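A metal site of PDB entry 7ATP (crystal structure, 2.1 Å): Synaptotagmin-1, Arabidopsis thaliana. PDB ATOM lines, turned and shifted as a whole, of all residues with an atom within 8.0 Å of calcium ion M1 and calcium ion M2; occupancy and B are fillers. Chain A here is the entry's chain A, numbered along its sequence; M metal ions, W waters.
The backbone NH (N) of Asp 80 sits close to the side-chain sulfur (SD) of Met 90 (3.7 Å). The backbone NH (N) of Lys 52 sits at hydrogen-bond distance from the side-chain carboxylate (OD1) of Asp 30, at 2.9 Å. The backbone carbonyl oxygen (O) of Gly 28 is in hydrogen-bond range of the backbone NH (N) of Lys 23.
Within 4 Å of calcium ion M1: Lys 23, Asp 24, Asp 80, Glu 82 and Glu 88.
Five residues have an atom within 4 Å of calcium ion M2: Asp 24, Asp 30, Asp 80, Trp 81 and Glu 82. The nearest printed residue that does not touch calcium ion M2 is Ala 29 (4.6 Å).
Calcium ion M1 is bound by the side-chain carboxylate (OE2) of Glu 88, the side-chain carboxylate (OE1) of Glu 82, the side-chain carboxylate (OD1) of Asp 24, water W2, the backbone carbonyl oxygen (O) of Lys 23, the side-chain carboxylate (OD2) of Asp 80 and the side-chain carboxylate (OE2) of Glu 82.
Calcium ion M2 is bound by OD2 of Asp 24, water W1, OD1 of Asp 80, OE2 of Glu 82, OD2 of Asp 30, OD1 of Asp 24 and O of Trp 81. Calcium ion M2 has seven donor atoms within binding distance. Slightly farther from calcium ion M2 lies OD2 of Asp 80 (3.0 Å).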
ATOM      1  N   LYS A  22      10.929  29.396 -11.347  1.00  0.00           N
ATOM      2  CA  LYS A  22       9.655  29.322 -10.653  1.00  0.00           C
ATOM      3  C   LYS A  22       8.534  29.488 -11.672  1.00  0.00           C
ATOM      4  O   LYS A  22       8.555  30.400 -12.495  1.00  0.00           O
ATOM      5  CB  LYS A  22       9.567  30.398  -9.583  1.00  0.00           C
ATOM      6  CG  LYS A  22      10.435  30.120  -8.364  1.00  0.00           C
ATOM      7  CD  LYS A  22      10.287  31.218  -7.302  1.00  0.00           C
ATOM      8  CE  LYS A  22      11.024  30.865  -6.003  1.00  0.00           C
ATOM      9  NZ  LYS A  22      10.705  31.808  -4.889  1.00  0.00           N
ATOM     10  N   LYS A  23       7.582  28.572 -11.641  1.00  0.00           N
ATOM     11  CA  LYS A  23       6.485  28.647 -12.583  1.00  0.00           C
ATOM     12  C   LYS A  23       5.133  28.495 -11.913  1.00  0.00           C
ATOM     13  O   LYS A  23       4.102  28.498 -12.603  1.00  0.00           O
ATOM     14  CB  LYS A  23       6.668  27.597 -13.682  1.00  0.00           C
ATOM     15  CG  LYS A  23       7.818  27.910 -14.620  1.00  0.00           C
ATOM     16  CD  LYS A  23       7.367  27.867 -16.081  1.00  0.00           C
ATOM     17  CE  LYS A  23       7.824  29.093 -16.860  1.00  0.00           C
ATOM     18  NZ  LYS A  23       9.238  29.448 -16.572  1.00  0.00           N
ATOM     19  N   ASP A  24       5.090  28.385 -10.589  1.00  0.00           N
ATOM     20  CA  ASP A  24       3.843  28.260  -9.859  1.00  0.00           C
ATOM     21  C   ASP A  24       3.755  29.355  -8.821  1.00  0.00           C
ATOM     22  O   ASP A  24       4.766  29.859  -8.327  1.00  0.00           O
ATOM     23  CB  ASP A  24       3.707  26.914  -9.156  1.00  0.00           C
ATOM     24  CG  ASP A  24       3.335  25.795 -10.096  1.00  0.00           C
ATOM     25  OD1 ASP A  24       2.750  26.121 -11.155  1.00  0.00           O
ATOM     26  OD2 ASP A  24       3.622  24.616  -9.775  1.00  0.00           O
ATOM     27  N   LEU A  25       2.509  29.687  -8.464  1.00  0.00           N
ATOM     28  CA  LEU A  25       2.262  30.663  -7.409  1.00  0.00           C
ATOM     29  C   LEU A  25       3.012  30.296  -6.133  1.00  0.00           C
ATOM     30  O   LEU A  25       3.562  31.166  -5.456  1.00  0.00           O
ATOM     31  CB  LEU A  25       0.770  30.761  -7.133  1.00  0.00           C
ATOM     32  CG  LEU A  25       0.329  32.026  -6.417  1.00  0.00           C
ATOM     33  CD1 LEU A  25       0.842  33.239  -7.180  1.00  0.00           C
ATOM     34  CD2 LEU A  25      -1.192  32.027  -6.332  1.00  0.00           C
ATOM     35  N   MET A  26       3.060  29.009  -5.800  1.00  0.00           N
ATOM     36  CA  MET A  26       3.829  28.536  -4.662  1.00  0.00           C
ATOM     37  C   MET A  26       4.243  27.091  -4.882  1.00  0.00           C
ATOM     38  O   MET A  26       3.479  26.294  -5.461  1.00  0.00           O
ATOM     39  CB  MET A  26       3.059  28.674  -3.351  1.00  0.00           C
ATOM     40  CG  MET A  26       1.967  27.661  -3.143  1.00  0.00           C
ATOM     41  SD  MET A  26       0.916  28.162  -1.764  1.00  0.00           S
ATOM     42  CE  MET A  26      -0.208  29.309  -2.562  1.00  0.00           C
ATOM     43  N   GLY A  27       5.445  26.763  -4.428  1.00  0.00           N
ATOM     44  CA  GLY A  27       6.011  25.449  -4.561  1.00  0.00           C
ATOM     45  C   GLY A  27       7.072  25.329  -5.631  1.00  0.00           C
ATOM     46  O   GLY A  27       7.721  24.275  -5.729  1.00  0.00           O
ATOM     47  N   GLY A  28       7.274  26.369  -6.438  1.00  0.00           N
ATOM     48  CA  GLY A  28       8.289  26.378  -7.462  1.00  0.00           C
ATOM     49  C   GLY A  28       7.727  26.011  -8.822  1.00  0.00           C
ATOM     50  O   GLY A  28       7.450  26.889  -9.651  1.00  0.00           O
ATOM     51  N   ALA A  29       7.573  24.706  -9.042  1.00  0.00           N
ATOM     52  CA  ALA A  29       7.100  24.118 -10.282  1.00  0.00           C
ATOM     53  C   ALA A  29       6.933  22.633 -10.012  1.00  0.00           C
ATOM     54  O   ALA A  29       7.377  22.104  -8.989  1.00  0.00           O
ATOM     55  CB  ALA A  29       8.069  24.357 -11.449  1.00  0.00           C
ATOM     56  N   ASP A  30       6.289  21.943 -10.942  1.00  0.00           N
ATOM     57  CA  ASP A  30       6.098  20.498 -10.868  1.00  0.00           C
ATOM     58  C   ASP A  30       6.685  19.904 -12.129  1.00  0.00           C
ATOM     59  O   ASP A  30       5.941  19.520 -13.045  1.00  0.00           O
ATOM     60  CB  ASP A  30       4.612  20.183 -10.704  1.00  0.00           C
ATOM     61  CG  ASP A  30       3.936  21.073  -9.656  1.00  0.00           C
ATOM     62  OD1 ASP A  30       4.266  20.944  -8.455  1.00  0.00           O
ATOM     63  OD2 ASP A  30       3.087  21.939  -9.988  1.00  0.00           O
ATOM     64  N   PRO A  31       8.015  19.841 -12.230  1.00  0.00           N
ATOM     65  CA  PRO A  31       8.630  19.492 -13.507  1.00  0.00           C
ATOM     66  C   PRO A  31       8.432  18.031 -13.838  1.00  0.00           C
ATOM     67  O   PRO A  31       8.362  17.181 -12.962  1.00  0.00           O
ATOM     68  CB  PRO A  31      10.110  19.824 -13.298  1.00  0.00           C
ATOM     69  CG  PRO A  31      10.296  19.778 -11.845  1.00  0.00           C
ATOM     70  CD  PRO A  31       9.013  20.311 -11.265  1.00  0.00           C
ATOM     71  N   VAL A  49       6.348  13.150 -12.474  1.00  0.00           N
ATOM     72  CA  VAL A  49       6.260  14.550 -12.060  1.00  0.00           C
ATOM     73  C   VAL A  49       6.886  14.690 -10.685  1.00  0.00           C
ATOM     74  O   VAL A  49       6.601  13.905  -9.778  1.00  0.00           O
ATOM     75  CB  VAL A  49       4.793  15.021 -11.998  1.00  0.00           C
ATOM     76  CG1 VAL A  49       4.750  16.462 -11.432  1.00  0.00           C
ATOM     77  CG2 VAL A  49       4.175  14.966 -13.331  1.00  0.00           C
ATOM     78  N   HIS A  51       6.609  16.957  -7.925  1.00  0.00           N
ATOM     79  CA  HIS A  51       5.838  18.089  -7.429  1.00  0.00           C
ATOM     80  C   HIS A  51       6.686  19.009  -6.576  1.00  0.00           C
ATOM     81  O   HIS A  51       7.502  18.565  -5.769  1.00  0.00           O
ATOM     82  CB  HIS A  51       4.670  17.605  -6.597  1.00  0.00           C
ATOM     83  CG  HIS A  51       3.690  16.817  -7.368  1.00  0.00           C
ATOM     84  ND1 HIS A  51       2.812  17.385  -8.263  1.00  0.00           N
ATOM     85  CD2 HIS A  51       3.433  15.489  -7.377  1.00  0.00           C
ATOM     86  CE1 HIS A  51       2.070  16.437  -8.807  1.00  0.00           C
ATOM     87  NE2 HIS A  51       2.431  15.281  -8.293  1.00  0.00           N
ATOM     88  N   LYS A  52       6.448  20.313  -6.727  1.00  0.00           N
ATOM     89  CA  LYS A  52       6.995  21.317  -5.825  1.00  0.00           C
ATOM     90  C   LYS A  52       8.507  21.152  -5.677  1.00  0.00           C
ATOM     91  O   LYS A  52       9.060  21.086  -4.580  1.00  0.00           O
ATOM     92  CB  LYS A  52       6.265  21.261  -4.480  1.00  0.00           C
ATOM     93  CG  LYS A  52       4.752  21.602  -4.647  1.00  0.00           C
ATOM     94  CD  LYS A  52       3.974  21.522  -3.341  1.00  0.00           C
ATOM     95  CE  LYS A  52       2.468  21.658  -3.596  1.00  0.00           C
ATOM     96  NZ  LYS A  52       2.214  22.812  -4.500  1.00  0.00           N
ATOM     97  N   TYR A  79       8.523  20.366 -18.755  1.00  0.00           N
ATOM     98  CA  TYR A  79       7.227  20.969 -18.532  1.00  0.00           C
ATOM     99  C   TYR A  79       6.908  21.011 -17.048  1.00  0.00           C
ATOM    100  O   TYR A  79       7.371  20.176 -16.250  1.00  0.00           O
ATOM    101  CB  TYR A  79       6.117  20.206 -19.245  1.00  0.00           C
ATOM    102  CG  TYR A  79       6.149  20.257 -20.750  1.00  0.00           C
ATOM    103  CD1 TYR A  79       5.538  21.296 -21.444  1.00  0.00           C
ATOM    104  CD2 TYR A  79       6.725  19.226 -21.489  1.00  0.00           C
ATOM    105  CE1 TYR A  79       5.539  21.329 -22.832  1.00  0.00           C
ATOM    106  CE2 TYR A  79       6.728  19.246 -22.872  1.00  0.00           C
ATOM    107  CZ  TYR A  79       6.134  20.304 -23.546  1.00  0.00           C
ATOM    108  OH  TYR A  79       6.145  20.317 -24.930  1.00  0.00           O
ATOM    109  N   ASP A  80       6.098  21.997 -16.682  1.00  0.00           N
ATOM    110  CA  ASP A  80       5.556  22.142 -15.334  1.00  0.00           C
ATOM    111  C   ASP A  80       4.095  21.684 -15.329  1.00  0.00           C
ATOM    112  O   ASP A  80       3.225  22.355 -15.895  1.00  0.00           O
ATOM    113  CB  ASP A  80       5.706  23.577 -14.875  1.00  0.00           C
ATOM    114  CG  ASP A  80       4.787  23.929 -13.713  1.00  0.00           C
ATOM    115  OD1 ASP A  80       4.641  23.106 -12.780  1.00  0.00           O
ATOM    116  OD2 ASP A  80       4.249  25.037 -13.724  1.00  0.00           O
ATOM    117  N   TRP A  81       3.841  20.548 -14.692  1.00  0.00           N
ATOM    118  CA  TRP A  81       2.490  20.014 -14.643  1.00  0.00           C
ATOM    119  C   TRP A  81       1.569  21.003 -13.945  1.00  0.00           C
ATOM    120  O   TRP A  81       1.964  21.650 -12.968  1.00  0.00           O
ATOM    121  CB  TRP A  81       2.517  18.674 -13.909  1.00  0.00           C
ATOM    122  CG  TRP A  81       1.170  18.046 -13.524  1.00  0.00           C
ATOM    123  CD1 TRP A  81       0.467  17.116 -14.236  1.00  0.00           C
ATOM    124  CD2 TRP A  81       0.466  18.226 -12.285  1.00  0.00           C
ATOM    125  NE1 TRP A  81      -0.640  16.719 -13.516  1.00  0.00           N
ATOM    126  CE2 TRP A  81      -0.659  17.388 -12.318  1.00  0.00           C
ATOM    127  CE3 TRP A  81       0.702  18.978 -11.154  1.00  0.00           C
ATOM    128  CZ2 TRP A  81      -1.592  17.334 -11.275  1.00  0.00           C
ATOM    129  CZ3 TRP A  81      -0.217  18.909 -10.099  1.00  0.00           C
ATOM    130  CH2 TRP A  81      -1.349  18.099 -10.177  1.00  0.00           C
ATOM    131  N   GLU A  82       0.367  21.159 -14.451  1.00  0.00           N
ATOM    132  CA  GLU A  82      -0.596  22.057 -13.835  1.00  0.00           C
ATOM    133  C   GLU A  82      -1.769  21.277 -13.293  1.00  0.00           C
ATOM    134  O   GLU A  82      -2.179  20.247 -13.854  1.00  0.00           O
ATOM    135  CB  GLU A  82      -1.092  23.125 -14.818  1.00  0.00           C
ATOM    136  CG  GLU A  82       0.035  23.951 -15.419  1.00  0.00           C
ATOM    137  CD  GLU A  82       0.763  24.815 -14.393  1.00  0.00           C
ATOM    138  OE1 GLU A  82       0.785  26.060 -14.562  1.00  0.00           O
ATOM    139  OE2 GLU A  82       1.289  24.247 -13.400  1.00  0.00           O
ATOM    140  N   GLN A  83      -2.308  21.769 -12.174  1.00  0.00           N
ATOM    141  CA  GLN A  83      -3.482  21.146 -11.619  1.00  0.00           C
ATOM    142  C   GLN A  83      -4.674  21.371 -12.516  1.00  0.00           C
ATOM    143  O   GLN A  83      -5.584  20.546 -12.555  1.00  0.00           O
ATOM    144  CB  GLN A  83      -3.739  21.673 -10.227  1.00  0.00           C
ATOM    145  CG  GLN A  83      -2.583  21.356  -9.332  1.00  0.00           C
ATOM    146  CD  GLN A  83      -2.921  21.522  -7.895  1.00  0.00           C
ATOM    147  OE1 GLN A  83      -3.889  22.221  -7.577  1.00  0.00           O
ATOM    148  NE2 GLN A  83      -2.152  20.868  -7.008  1.00  0.00           N
ATOM    149  N   VAL A  84      -4.660  22.445 -13.290  1.00  0.00           N
ATOM    150  CA  VAL A  84      -5.756  22.742 -14.191  1.00  0.00           C
ATOM    151  C   VAL A  84      -5.164  23.138 -15.532  1.00  0.00           C
ATOM    152  O   VAL A  84      -4.261  23.980 -15.592  1.00  0.00           O
ATOM    153  CB  VAL A  84      -6.666  23.839 -13.629  1.00  0.00           C
ATOM    154  CG1 VAL A  84      -7.715  24.192 -14.658  1.00  0.00           C
ATOM    155  CG2 VAL A  84      -7.305  23.358 -12.346  1.00  0.00           C
ATOM    156  N   ASN A  86      -3.341  22.461 -19.211  1.00  0.00           N
ATOM    157  CA  ASN A  86      -2.254  21.674 -19.719  1.00  0.00           C
ATOM    158  C   ASN A  86      -0.940  22.093 -19.084  1.00  0.00           C
ATOM    159  O   ASN A  86      -0.810  23.230 -18.613  1.00  0.00           O
ATOM    160  CB  ASN A  86      -2.160  21.821 -21.248  1.00  0.00           C
ATOM    161  CG  ASN A  86      -3.072  20.841 -21.975  1.00  0.00           C
ATOM    162  OD1 ASN A  86      -3.342  19.748 -21.469  1.00  0.00           O
ATOM    163  ND2 ASN A  86      -3.539  21.230 -23.161  1.00  0.00           N
ATOM    164  N   PRO A  87       0.031  21.198 -19.030  1.00  0.00           N
ATOM    165  CA  PRO A  87       1.345  21.564 -18.502  1.00  0.00           C
ATOM    166  C   PRO A  87       1.877  22.755 -19.275  1.00  0.00           C
ATOM    167  O   PRO A  87       1.503  22.953 -20.429  1.00  0.00           O
ATOM    168  CB  PRO A  87       2.190  20.303 -18.736  1.00  0.00           C
ATOM    169  CG  PRO A  87       1.188  19.200 -18.728  1.00  0.00           C
ATOM    170  CD  PRO A  87       0.003  19.785 -19.458  1.00  0.00           C
ATOM    171  N   GLU A  88       2.699  23.566 -18.622  1.00  0.00           N
ATOM    172  CA  GLU A  88       3.325  24.702 -19.283  1.00  0.00           C
ATOM    173  C   GLU A  88       4.800  24.434 -19.510  1.00  0.00           C
ATOM    174  O   GLU A  88       5.503  24.014 -18.592  1.00  0.00           O
ATOM    175  CB  GLU A  88       3.142  25.991 -18.480  1.00  0.00           C
ATOM    176  CG  GLU A  88       3.718  26.022 -17.105  1.00  0.00           C
ATOM    177  CD  GLU A  88       3.625  27.411 -16.482  1.00  0.00           C
ATOM    178  OE1 GLU A  88       4.050  28.392 -17.137  1.00  0.00           O
ATOM    179  OE2 GLU A  88       3.112  27.519 -15.343  1.00  0.00           O
ATOM    180  N   LYS A  89       5.231  24.666 -20.742  1.00  0.00           N
ATOM    181  CA  LYS A  89       6.623  24.469 -21.107  1.00  0.00           C
ATOM    182  C   LYS A  89       7.531  25.245 -20.156  1.00  0.00           C
ATOM    183  O   LYS A  89       7.178  26.343 -19.702  1.00  0.00           O
ATOM    184  CB  LYS A  89       6.865  24.918 -22.542  1.00  0.00           C
ATOM    185  CG  LYS A  89       8.288  24.726 -23.041  1.00  0.00           C
ATOM    186  CD  LYS A  89       8.611  23.248 -23.277  1.00  0.00           C
ATOM    187  CE  LYS A  89       8.981  22.996 -24.736  1.00  0.00           C
ATOM    188  NZ  LYS A  89       7.890  23.446 -25.662  1.00  0.00           N
ATOM    189  N   MET A  90       8.681  24.659 -19.836  1.00  0.00           N
ATOM    190  CA  MET A  90       9.715  25.340 -19.076  1.00  0.00           C
ATOM    191  C   MET A  90      11.031  25.474 -19.841  1.00  0.00           C
ATOM    192  O   MET A  90      11.985  26.062 -19.312  1.00  0.00           O
ATOM    193  CB  MET A  90       9.973  24.612 -17.751  1.00  0.00           C
ATOM    194  CG  MET A  90       8.814  24.656 -16.816  1.00  0.00           C
ATOM    195  SD  MET A  90       9.179  23.622 -15.424  1.00  0.00           S
ATOM    196  CE  MET A  90      10.248  24.659 -14.437  1.00  0.00           C
HETATM  197 CA    CA M   1       2.528  26.759 -13.332  1.00  0.00          CA
HETATM  198 CA    CA M   2       2.690  23.676 -11.600  1.00  0.00          CA
HETATM  199  O   HOH W   1       0.817  23.678 -10.341  1.00  0.00           O
HETATM  200  O   HOH W   2       0.839  28.166 -12.469  1.00  0.00           O
